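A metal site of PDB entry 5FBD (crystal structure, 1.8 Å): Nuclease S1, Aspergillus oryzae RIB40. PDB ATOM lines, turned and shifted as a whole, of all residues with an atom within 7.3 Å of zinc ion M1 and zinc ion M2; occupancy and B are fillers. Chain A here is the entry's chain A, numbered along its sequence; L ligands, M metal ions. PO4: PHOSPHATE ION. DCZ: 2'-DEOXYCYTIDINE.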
ATOM      1  N   TRP A   1      -2.244  14.628  12.519  1.00  0.00           N
ATOM      2  CA  TRP A   1      -1.969  13.361  13.169  1.00  0.00           C
ATOM      3  C   TRP A   1      -0.488  13.319  13.403  1.00  0.00           C
ATOM      4  O   TRP A   1       0.257  14.001  12.718  1.00  0.00           O
ATOM      5  CB  TRP A   1      -2.375  12.154  12.316  1.00  0.00           C
ATOM      6  CG  TRP A   1      -3.801  12.193  11.876  1.00  0.00           C
ATOM      7  CD1 TRP A   1      -4.251  12.545  10.652  1.00  0.00           C
ATOM      8  CD2 TRP A   1      -4.956  11.972  12.695  1.00  0.00           C
ATOM      9  NE1 TRP A   1      -5.625  12.476  10.622  1.00  0.00           N
ATOM     10  CE2 TRP A   1      -6.083  12.115  11.858  1.00  0.00           C
ATOM     11  CE3 TRP A   1      -5.142  11.603  14.042  1.00  0.00           C
ATOM     12  CZ2 TRP A   1      -7.389  12.006  12.329  1.00  0.00           C
ATOM     13  CZ3 TRP A   1      -6.413  11.445  14.509  1.00  0.00           C
ATOM     14  CH2 TRP A   1      -7.563  11.624  13.634  1.00  0.00           C
ATOM     15  N   GLY A   2      -0.079  12.452  14.299  1.00  0.00           N
ATOM     16  CA  GLY A   2       1.320  12.045  14.428  1.00  0.00           C
ATOM     17  C   GLY A   2       1.625  11.095  13.300  1.00  0.00           C
ATOM     18  O   GLY A   2       0.789  10.818  12.407  1.00  0.00           O
ATOM     19  N   ASN A   3       2.846  10.606  13.336  1.00  0.00           N
ATOM     20  CA  ASN A   3       3.373   9.831  12.238  1.00  0.00           C
ATOM     21  C   ASN A   3       2.514   8.623  11.962  1.00  0.00           C
ATOM     22  O   ASN A   3       2.218   8.343  10.812  1.00  0.00           O
ATOM     23  CB  ASN A   3       4.824   9.411  12.485  1.00  0.00           C
ATOM     24  CG  ASN A   3       5.798  10.565  12.447  1.00  0.00           C
ATOM     25  OD1 ASN A   3       5.523  11.664  11.965  1.00  0.00           O
ATOM     26  ND2 ASN A   3       6.986  10.314  12.971  1.00  0.00           N
ATOM     27  N   GLY A   5      -0.697   8.038  12.490  1.00  0.00           N
ATOM     28  CA  GLY A   5      -1.922   8.378  11.797  1.00  0.00           C
ATOM     29  C   GLY A   5      -1.727   8.713  10.347  1.00  0.00           C
ATOM     30  O   GLY A   5      -2.529   8.280   9.506  1.00  0.00           O
ATOM     31  N   HIS A   6      -0.675   9.458  10.014  1.00  0.00           N
ATOM     32  CA  HIS A   6      -0.421   9.806   8.617  1.00  0.00           C
ATOM     33  C   HIS A   6      -0.114   8.583   7.768  1.00  0.00           C
ATOM     34  O   HIS A   6      -0.529   8.507   6.587  1.00  0.00           O
ATOM     35  CB  HIS A   6       0.724  10.809   8.502  1.00  0.00           C
ATOM     36  CG  HIS A   6       0.291  12.189   8.870  1.00  0.00           C
ATOM     37  ND1 HIS A   6      -0.567  12.915   8.079  1.00  0.00           N
ATOM     38  CD2 HIS A   6       0.514  12.940   9.987  1.00  0.00           C
ATOM     39  CE1 HIS A   6      -0.863  14.067   8.681  1.00  0.00           C
ATOM     40  NE2 HIS A   6      -0.253  14.081   9.857  1.00  0.00           N
ATOM     41  N   ALA A  41       4.473  10.193   3.848  1.00  0.00           N
ATOM     42  CA  ALA A  41       3.334  10.794   4.504  1.00  0.00           C
ATOM     43  C   ALA A  41       3.668  11.694   5.668  1.00  0.00           C
ATOM     44  O   ALA A  41       2.793  12.446   6.081  1.00  0.00           O
ATOM     45  CB  ALA A  41       2.352   9.728   4.965  1.00  0.00           C
ATOM     46  N   THR A  42       4.896  11.600   6.204  1.00  0.00           N
ATOM     47  CA  THR A  42       5.311  12.374   7.401  1.00  0.00           C
ATOM     48  C   THR A  42       6.246  13.529   7.001  1.00  0.00           C
ATOM     49  O   THR A  42       6.490  14.401   7.804  1.00  0.00           O
ATOM     50  CB  THR A  42       6.027  11.495   8.459  1.00  0.00           C
ATOM     51  OG1 THR A  42       7.241  11.002   7.895  1.00  0.00           O
ATOM     52  CG2 THR A  42       5.149  10.343   8.881  1.00  0.00           C
ATOM     53  N   ALA A  44       6.176  16.346   5.416  1.00  0.00           N
ATOM     54  CA  ALA A  44       5.757  17.751   5.586  1.00  0.00           C
ATOM     55  C   ALA A  44       5.921  18.227   7.026  1.00  0.00           C
ATOM     56  O   ALA A  44       6.230  19.406   7.244  1.00  0.00           O
ATOM     57  CB  ALA A  44       4.331  17.984   5.078  1.00  0.00           C
ATOM     58  N   ASP A  45       5.866  17.296   7.994  1.00  0.00           N
ATOM     59  CA  ASP A  45       5.938  17.667   9.418  1.00  0.00           C
ATOM     60  C   ASP A  45       7.329  17.947   9.901  1.00  0.00           C
ATOM     61  O   ASP A  45       7.496  18.699  10.815  1.00  0.00           O
ATOM     62  CB  ASP A  45       5.264  16.626  10.322  1.00  0.00           C
ATOM     63  CG  ASP A  45       3.778  16.868  10.480  1.00  0.00           C
ATOM     64  OD1 ASP A  45       3.253  17.960  10.054  1.00  0.00           O
ATOM     65  OD2 ASP A  45       3.118  15.955  11.008  1.00  0.00           O
ATOM     66  N   LYS A  48       8.591  21.464   7.528  1.00  0.00           N
ATOM     67  CA  LYS A  48       8.157  22.761   7.998  1.00  0.00           C
ATOM     68  C   LYS A  48       9.005  23.431   9.053  1.00  0.00           C
ATOM     69  O   LYS A  48       8.810  24.635   9.324  1.00  0.00           O
ATOM     70  CB  LYS A  48       6.712  22.723   8.502  1.00  0.00           C
ATOM     71  CG  LYS A  48       6.507  21.942   9.812  1.00  0.00           C
ATOM     72  CD  LYS A  48       5.046  21.642  10.006  1.00  0.00           C
ATOM     73  CE  LYS A  48       4.717  20.968  11.332  1.00  0.00           C
ATOM     74  NZ  LYS A  48       3.294  20.527  11.430  1.00  0.00           N
ATOM     75  N   LYS A  57       4.525  25.790   7.229  1.00  0.00           N
ATOM     76  CA  LYS A  57       3.921  25.475   8.533  1.00  0.00           C
ATOM     77  C   LYS A  57       2.407  25.727   8.567  1.00  0.00           C
ATOM     78  O   LYS A  57       1.677  24.920   9.110  1.00  0.00           O
ATOM     79  CB  LYS A  57       4.662  26.209   9.648  1.00  0.00           C
ATOM     80  CG  LYS A  57       4.280  25.747  11.031  1.00  0.00           C
ATOM     81  CD  LYS A  57       5.154  26.428  12.081  1.00  0.00           C
ATOM     82  CE  LYS A  57       6.610  26.398  11.654  1.00  0.00           C
ATOM     83  NZ  LYS A  57       7.443  26.982  12.731  1.00  0.00           N
ATOM     84  N   TYR A  59       0.168  25.480   6.343  1.00  0.00           N
ATOM     85  CA  TYR A  59      -0.571  24.568   5.502  1.00  0.00           C
ATOM     86  C   TYR A  59      -1.127  23.341   6.187  1.00  0.00           C
ATOM     87  O   TYR A  59      -1.794  22.564   5.522  1.00  0.00           O
ATOM     88  CB  TYR A  59       0.267  24.094   4.320  1.00  0.00           C
ATOM     89  CG  TYR A  59       0.864  25.198   3.427  1.00  0.00           C
ATOM     90  CD1 TYR A  59       0.503  26.525   3.541  1.00  0.00           C
ATOM     91  CD2 TYR A  59       1.833  24.870   2.504  1.00  0.00           C
ATOM     92  CE1 TYR A  59       1.073  27.500   2.761  1.00  0.00           C
ATOM     93  CE2 TYR A  59       2.395  25.822   1.675  1.00  0.00           C
ATOM     94  CZ  TYR A  59       2.005  27.132   1.800  1.00  0.00           C
ATOM     95  OH  TYR A  59       2.564  28.107   0.963  1.00  0.00           O
ATOM     96  N   HIS A  60      -0.888  23.150   7.458  1.00  0.00           N
ATOM     97  CA  HIS A  60      -1.304  21.920   8.144  1.00  0.00           C
ATOM     98  C   HIS A  60      -2.699  21.979   8.745  1.00  0.00           C
ATOM     99  O   HIS A  60      -3.209  20.951   9.243  1.00  0.00           O
ATOM    100  CB  HIS A  60      -0.253  21.487   9.139  1.00  0.00           C
ATOM    101  CG  HIS A  60       1.029  21.077   8.497  1.00  0.00           C
ATOM    102  ND1 HIS A  60       1.502  19.772   8.533  1.00  0.00           N
ATOM    103  CD2 HIS A  60       1.898  21.775   7.723  1.00  0.00           C
ATOM    104  CE1 HIS A  60       2.658  19.721   7.909  1.00  0.00           C
ATOM    105  NE2 HIS A  60       2.867  20.903   7.341  1.00  0.00           N
ATOM    106  N   PHE A  61      -3.281  23.172   8.793  1.00  0.00           N
ATOM    107  CA  PHE A  61      -4.539  23.341   9.496  1.00  0.00           C
ATOM    108  C   PHE A  61      -5.321  24.521   8.931  1.00  0.00           C
ATOM    109  O   PHE A  61      -4.829  25.287   8.070  1.00  0.00           O
ATOM    110  CB  PHE A  61      -4.280  23.556  11.001  1.00  0.00           C
ATOM    111  CG  PHE A  61      -3.263  24.643  11.279  1.00  0.00           C
ATOM    112  CD1 PHE A  61      -3.637  25.957  11.334  1.00  0.00           C
ATOM    113  CD2 PHE A  61      -1.942  24.326  11.435  1.00  0.00           C
ATOM    114  CE1 PHE A  61      -2.699  26.964  11.603  1.00  0.00           C
ATOM    115  CE2 PHE A  61      -0.987  25.328  11.657  1.00  0.00           C
ATOM    116  CZ  PHE A  61      -1.385  26.643  11.748  1.00  0.00           C
ATOM    117  N   HIS A 115      -0.083  14.145   2.958  1.00  0.00           N
ATOM    118  CA  HIS A 115      -0.024  14.541   4.370  1.00  0.00           C
ATOM    119  C   HIS A 115      -1.262  15.364   4.778  1.00  0.00           C
ATOM    120  O   HIS A 115      -1.846  15.107   5.826  1.00  0.00           O
ATOM    121  CB  HIS A 115       1.199  15.444   4.607  1.00  0.00           C
ATOM    122  CG  HIS A 115       1.398  15.777   6.048  1.00  0.00           C
ATOM    123  ND1 HIS A 115       2.015  14.910   6.939  1.00  0.00           N
ATOM    124  CD2 HIS A 115       0.991  16.821   6.770  1.00  0.00           C
ATOM    125  CE1 HIS A 115       2.028  15.467   8.128  1.00  0.00           C
ATOM    126  NE2 HIS A 115       1.398  16.622   8.051  1.00  0.00           N
ATOM    127  N   ILE A 116      -1.558  16.382   3.983  1.00  0.00           N
ATOM    128  CA  ILE A 116      -2.568  17.386   4.347  1.00  0.00           C
ATOM    129  C   ILE A 116      -3.967  16.827   4.282  1.00  0.00           C
ATOM    130  O   ILE A 116      -4.753  17.157   5.154  1.00  0.00           O
ATOM    131  CB  ILE A 116      -2.421  18.678   3.570  1.00  0.00           C
ATOM    132  CG1 ILE A 116      -1.057  19.290   3.963  1.00  0.00           C
ATOM    133  CG2 ILE A 116      -3.550  19.644   3.880  1.00  0.00           C
ATOM    134  CD1 ILE A 116      -0.557  20.411   3.132  1.00  0.00           C
ATOM    135  N   GLY A 118      -4.725  13.880   5.210  1.00  0.00           N
ATOM    136  CA  GLY A 118      -4.813  13.343   6.549  1.00  0.00           C
ATOM    137  C   GLY A 118      -5.028  14.396   7.639  1.00  0.00           C
ATOM    138  O   GLY A 118      -5.892  14.182   8.530  1.00  0.00           O
ATOM    139  N   ASP A 119      -4.229  15.505   7.639  1.00  0.00           N
ATOM    140  CA  ASP A 119      -4.363  16.539   8.706  1.00  0.00           C
ATOM    141  C   ASP A 119      -5.754  17.143   8.753  1.00  0.00           C
ATOM    142  O   ASP A 119      -6.265  17.400   9.809  1.00  0.00           O
ATOM    143  CB  ASP A 119      -3.326  17.673   8.548  1.00  0.00           C
ATOM    144  CG  ASP A 119      -2.023  17.400   9.303  1.00  0.00           C
ATOM    145  OD1 ASP A 119      -2.037  16.502  10.152  1.00  0.00           O
ATOM    146  OD2 ASP A 119      -1.004  18.078   9.054  1.00  0.00           O
ATOM    147  N   ILE A 120      -6.372  17.360   7.582  1.00  0.00           N
ATOM    148  CA  ILE A 120      -7.736  17.915   7.501  1.00  0.00           C
ATOM    149  C   ILE A 120      -8.727  17.064   8.284  1.00  0.00           C
ATOM    150  O   ILE A 120      -9.657  17.583   8.889  1.00  0.00           O
ATOM    151  CB  ILE A 120      -8.142  18.094   6.060  1.00  0.00           C
ATOM    152  CG1 ILE A 120      -7.319  19.240   5.428  1.00  0.00           C
ATOM    153  CG2 ILE A 120      -9.641  18.354   5.911  1.00  0.00           C
ATOM    154  CD1 ILE A 120      -7.576  19.339   3.950  1.00  0.00           C
ATOM    155  N   GLN A 122      -8.174  15.460  11.100  1.00  0.00           N
ATOM    156  CA  GLN A 122      -7.939  15.521  12.523  1.00  0.00           C
ATOM    157  C   GLN A 122      -8.742  16.774  12.996  1.00  0.00           C
ATOM    158  O   GLN A 122      -8.419  17.875  12.604  1.00  0.00           O
ATOM    159  CB  GLN A 122      -6.439  15.632  12.851  1.00  0.00           C
ATOM    160  CG  GLN A 122      -6.047  15.137  14.238  1.00  0.00           C
ATOM    161  CD  GLN A 122      -6.456  16.051  15.393  1.00  0.00           C
ATOM    162  OE1 GLN A 122      -7.657  16.370  15.586  1.00  0.00           O
ATOM    163  NE2 GLN A 122      -5.484  16.472  16.207  1.00  0.00           N
ATOM    164  N   HIS A 125      -7.236  20.136  13.834  1.00  0.00           N
ATOM    165  CA  HIS A 125      -6.609  20.862  12.704  1.00  0.00           C
ATOM    166  C   HIS A 125      -7.609  21.712  11.924  1.00  0.00           C
ATOM    167  O   HIS A 125      -7.244  22.334  10.911  1.00  0.00           O
ATOM    168  CB  HIS A 125      -5.971  19.844  11.753  1.00  0.00           C
ATOM    169  CG  HIS A 125      -4.619  19.362  12.202  1.00  0.00           C
ATOM    170  ND1 HIS A 125      -3.464  19.691  11.530  1.00  0.00           N
ATOM    171  CD2 HIS A 125      -4.234  18.613  13.259  1.00  0.00           C
ATOM    172  CE1 HIS A 125      -2.420  19.222  12.174  1.00  0.00           C
ATOM    173  NE2 HIS A 125      -2.865  18.518  13.206  1.00  0.00           N
ATOM    174  N   HIS A 148      -4.343  18.713  21.731  1.00  0.00           N
ATOM    175  CA  HIS A 148      -3.908  18.442  20.373  1.00  0.00           C
ATOM    176  C   HIS A 148      -3.039  17.162  20.264  1.00  0.00           C
ATOM    177  O   HIS A 148      -3.289  16.291  19.390  1.00  0.00           O
ATOM    178  CB  HIS A 148      -3.196  19.651  19.814  1.00  0.00           C
ATOM    179  CG  HIS A 148      -2.962  19.549  18.334  1.00  0.00           C
ATOM    180  ND1 HIS A 148      -3.769  20.179  17.408  1.00  0.00           N
ATOM    181  CD2 HIS A 148      -2.065  18.831  17.619  1.00  0.00           C
ATOM    182  CE1 HIS A 148      -3.322  19.912  16.198  1.00  0.00           C
ATOM    183  NE2 HIS A 148      -2.303  19.091  16.298  1.00  0.00           N
ATOM    184  N   ASP A 152      -3.590  13.818  18.034  1.00  0.00           N
ATOM    185  CA  ASP A 152      -2.634  13.489  16.999  1.00  0.00           C
ATOM    186  C   ASP A 152      -1.969  12.174  17.243  1.00  0.00           C
ATOM    187  O   ASP A 152      -1.744  11.378  16.302  1.00  0.00           O
ATOM    188  CB  ASP A 152      -1.512  14.580  16.909  1.00  0.00           C
ATOM    189  CG  ASP A 152      -1.786  15.650  15.852  1.00  0.00           C
ATOM    190  OD1 ASP A 152      -2.875  15.748  15.239  1.00  0.00           O
ATOM    191  OD2 ASP A 152      -0.832  16.376  15.655  1.00  0.00           O
HETATM  192  P   PO4 L   1       0.780  18.011  12.676  1.00  0.00           P
HETATM  193  O1  PO4 L   1       0.050  16.702  12.612  1.00  0.00           O
HETATM  194  O2  PO4 L   1       0.824  18.823  11.405  1.00  0.00           O
HETATM  195  O3  PO4 L   1       0.104  18.704  13.836  1.00  0.00           O
HETATM  196  O4  PO4 L   1       2.239  17.788  13.099  1.00  0.00           O
HETATM  197  N1  DCZ L   2      -1.370  23.108  14.831  1.00  0.00           N
HETATM  198  C2  DCZ L   2      -2.728  23.166  14.509  1.00  0.00           C
HETATM  199  N3  DCZ L   2      -3.383  24.340  14.657  1.00  0.00           N
HETATM  200  C4  DCZ L   2      -2.718  25.425  15.120  1.00  0.00           C
HETATM  201  C5  DCZ L   2      -1.339  25.377  15.451  1.00  0.00           C
HETATM  202  C6  DCZ L   2      -0.725  24.211  15.302  1.00  0.00           C
HETATM  203  O2  DCZ L   2      -3.289  22.130  14.086  1.00  0.00           O
HETATM  204  N4  DCZ L   2      -3.375  26.551  15.244  1.00  0.00           N
HETATM  205  C1' DCZ L   2      -0.669  21.837  14.711  1.00  0.00           C
HETATM  206  C2' DCZ L   2       0.567  21.957  13.821  1.00  0.00           C
HETATM  207  C3' DCZ L   2       1.745  21.801  14.776  1.00  0.00           C
HETATM  208  C4' DCZ L   2       1.158  21.096  15.989  1.00  0.00           C
HETATM  209  O4' DCZ L   2      -0.231  21.478  16.022  1.00  0.00           O
HETATM  210  O3' DCZ L   2       2.661  20.896  14.168  1.00  0.00           O
HETATM  211  C5' DCZ L   2       1.813  21.434  17.315  1.00  0.00           C
HETATM  212  O5' DCZ L   2       2.144  22.839  17.398  1.00  0.00           O
HETATM  213 ZN    ZN M   1       0.991  18.130   9.538  1.00  0.00          ZN
HETATM  214 ZN    ZN M   2      -0.730  15.411  11.372  1.00  0.00          ZN
HETATM  215 ZN    ZN M   3      -1.486  18.059  14.680  1.00  0.00          ZN
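O1 of PO4 L1 binds zinc ion M2 (2.0 Å).
Zinc ion M2 is bound by N of Trp 1 (2.1 Å).
NE2 of His 6 is bound to zinc ion M2.
The side-chain carboxylate (OD1) of Asp 119 binds zinc ion M2 (2.1 Å).
O of Trp 1 binds zinc ion M2 (2.2 Å).
The side-chain amino group (NZ) of Lys 48 lies within hydrogen-bond range of an oxygen (O3') of DCZ L2, at 2.8 Å.
O4' of DCZ L2 sits close to NE2 of His 148, at 3.2 Å.
Four residues have an atom within 4 Å of zinc ion M2: Trp 1, His 6, Asp 45 and Asp 119.
Merely in contact with zinc ion M1: Lys 48 (3.8 Å).
Five residues have an atom within 4 Å of zinc ion M1: Asp 45, Lys 48, His 60, His 115 and Asp 119.
The nearest printed residue that does not touch zinc ion M1 is His 6 (4.2 Å).
NZ of Lys 48 lies close to ND1 of His 60, 3.5 Å away.
O of His 60 lies within hydrogen-bond range of ND1 of His 125 (2.6 Å).
N of Trp 1 lies close to OD1 of Asp 152 (3.0 Å).
The backbone carbonyl oxygen of Gly 118 sits at hydrogen-bond distance from the indole nitrogen of Trp 1 (2.7 Å).
O of His 115 sits close to ND1 of His 6 (3.4 Å).
ND1 of His 115 is in hydrogen-bond range of O of Ala 41, 2.7 Å away.
The side-chain carboxylate of Asp 45 sits close to the side-chain amino group of Lys 48, 2.9 Å away.
Zinc ion M1 is bound by ND1 of His 60, O2 of PO4 L1, OD2 of Asp 119, NE2 of His 115 and OD1 of Asp 45.
Zinc ion M1 has five donor atoms within binding distance.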
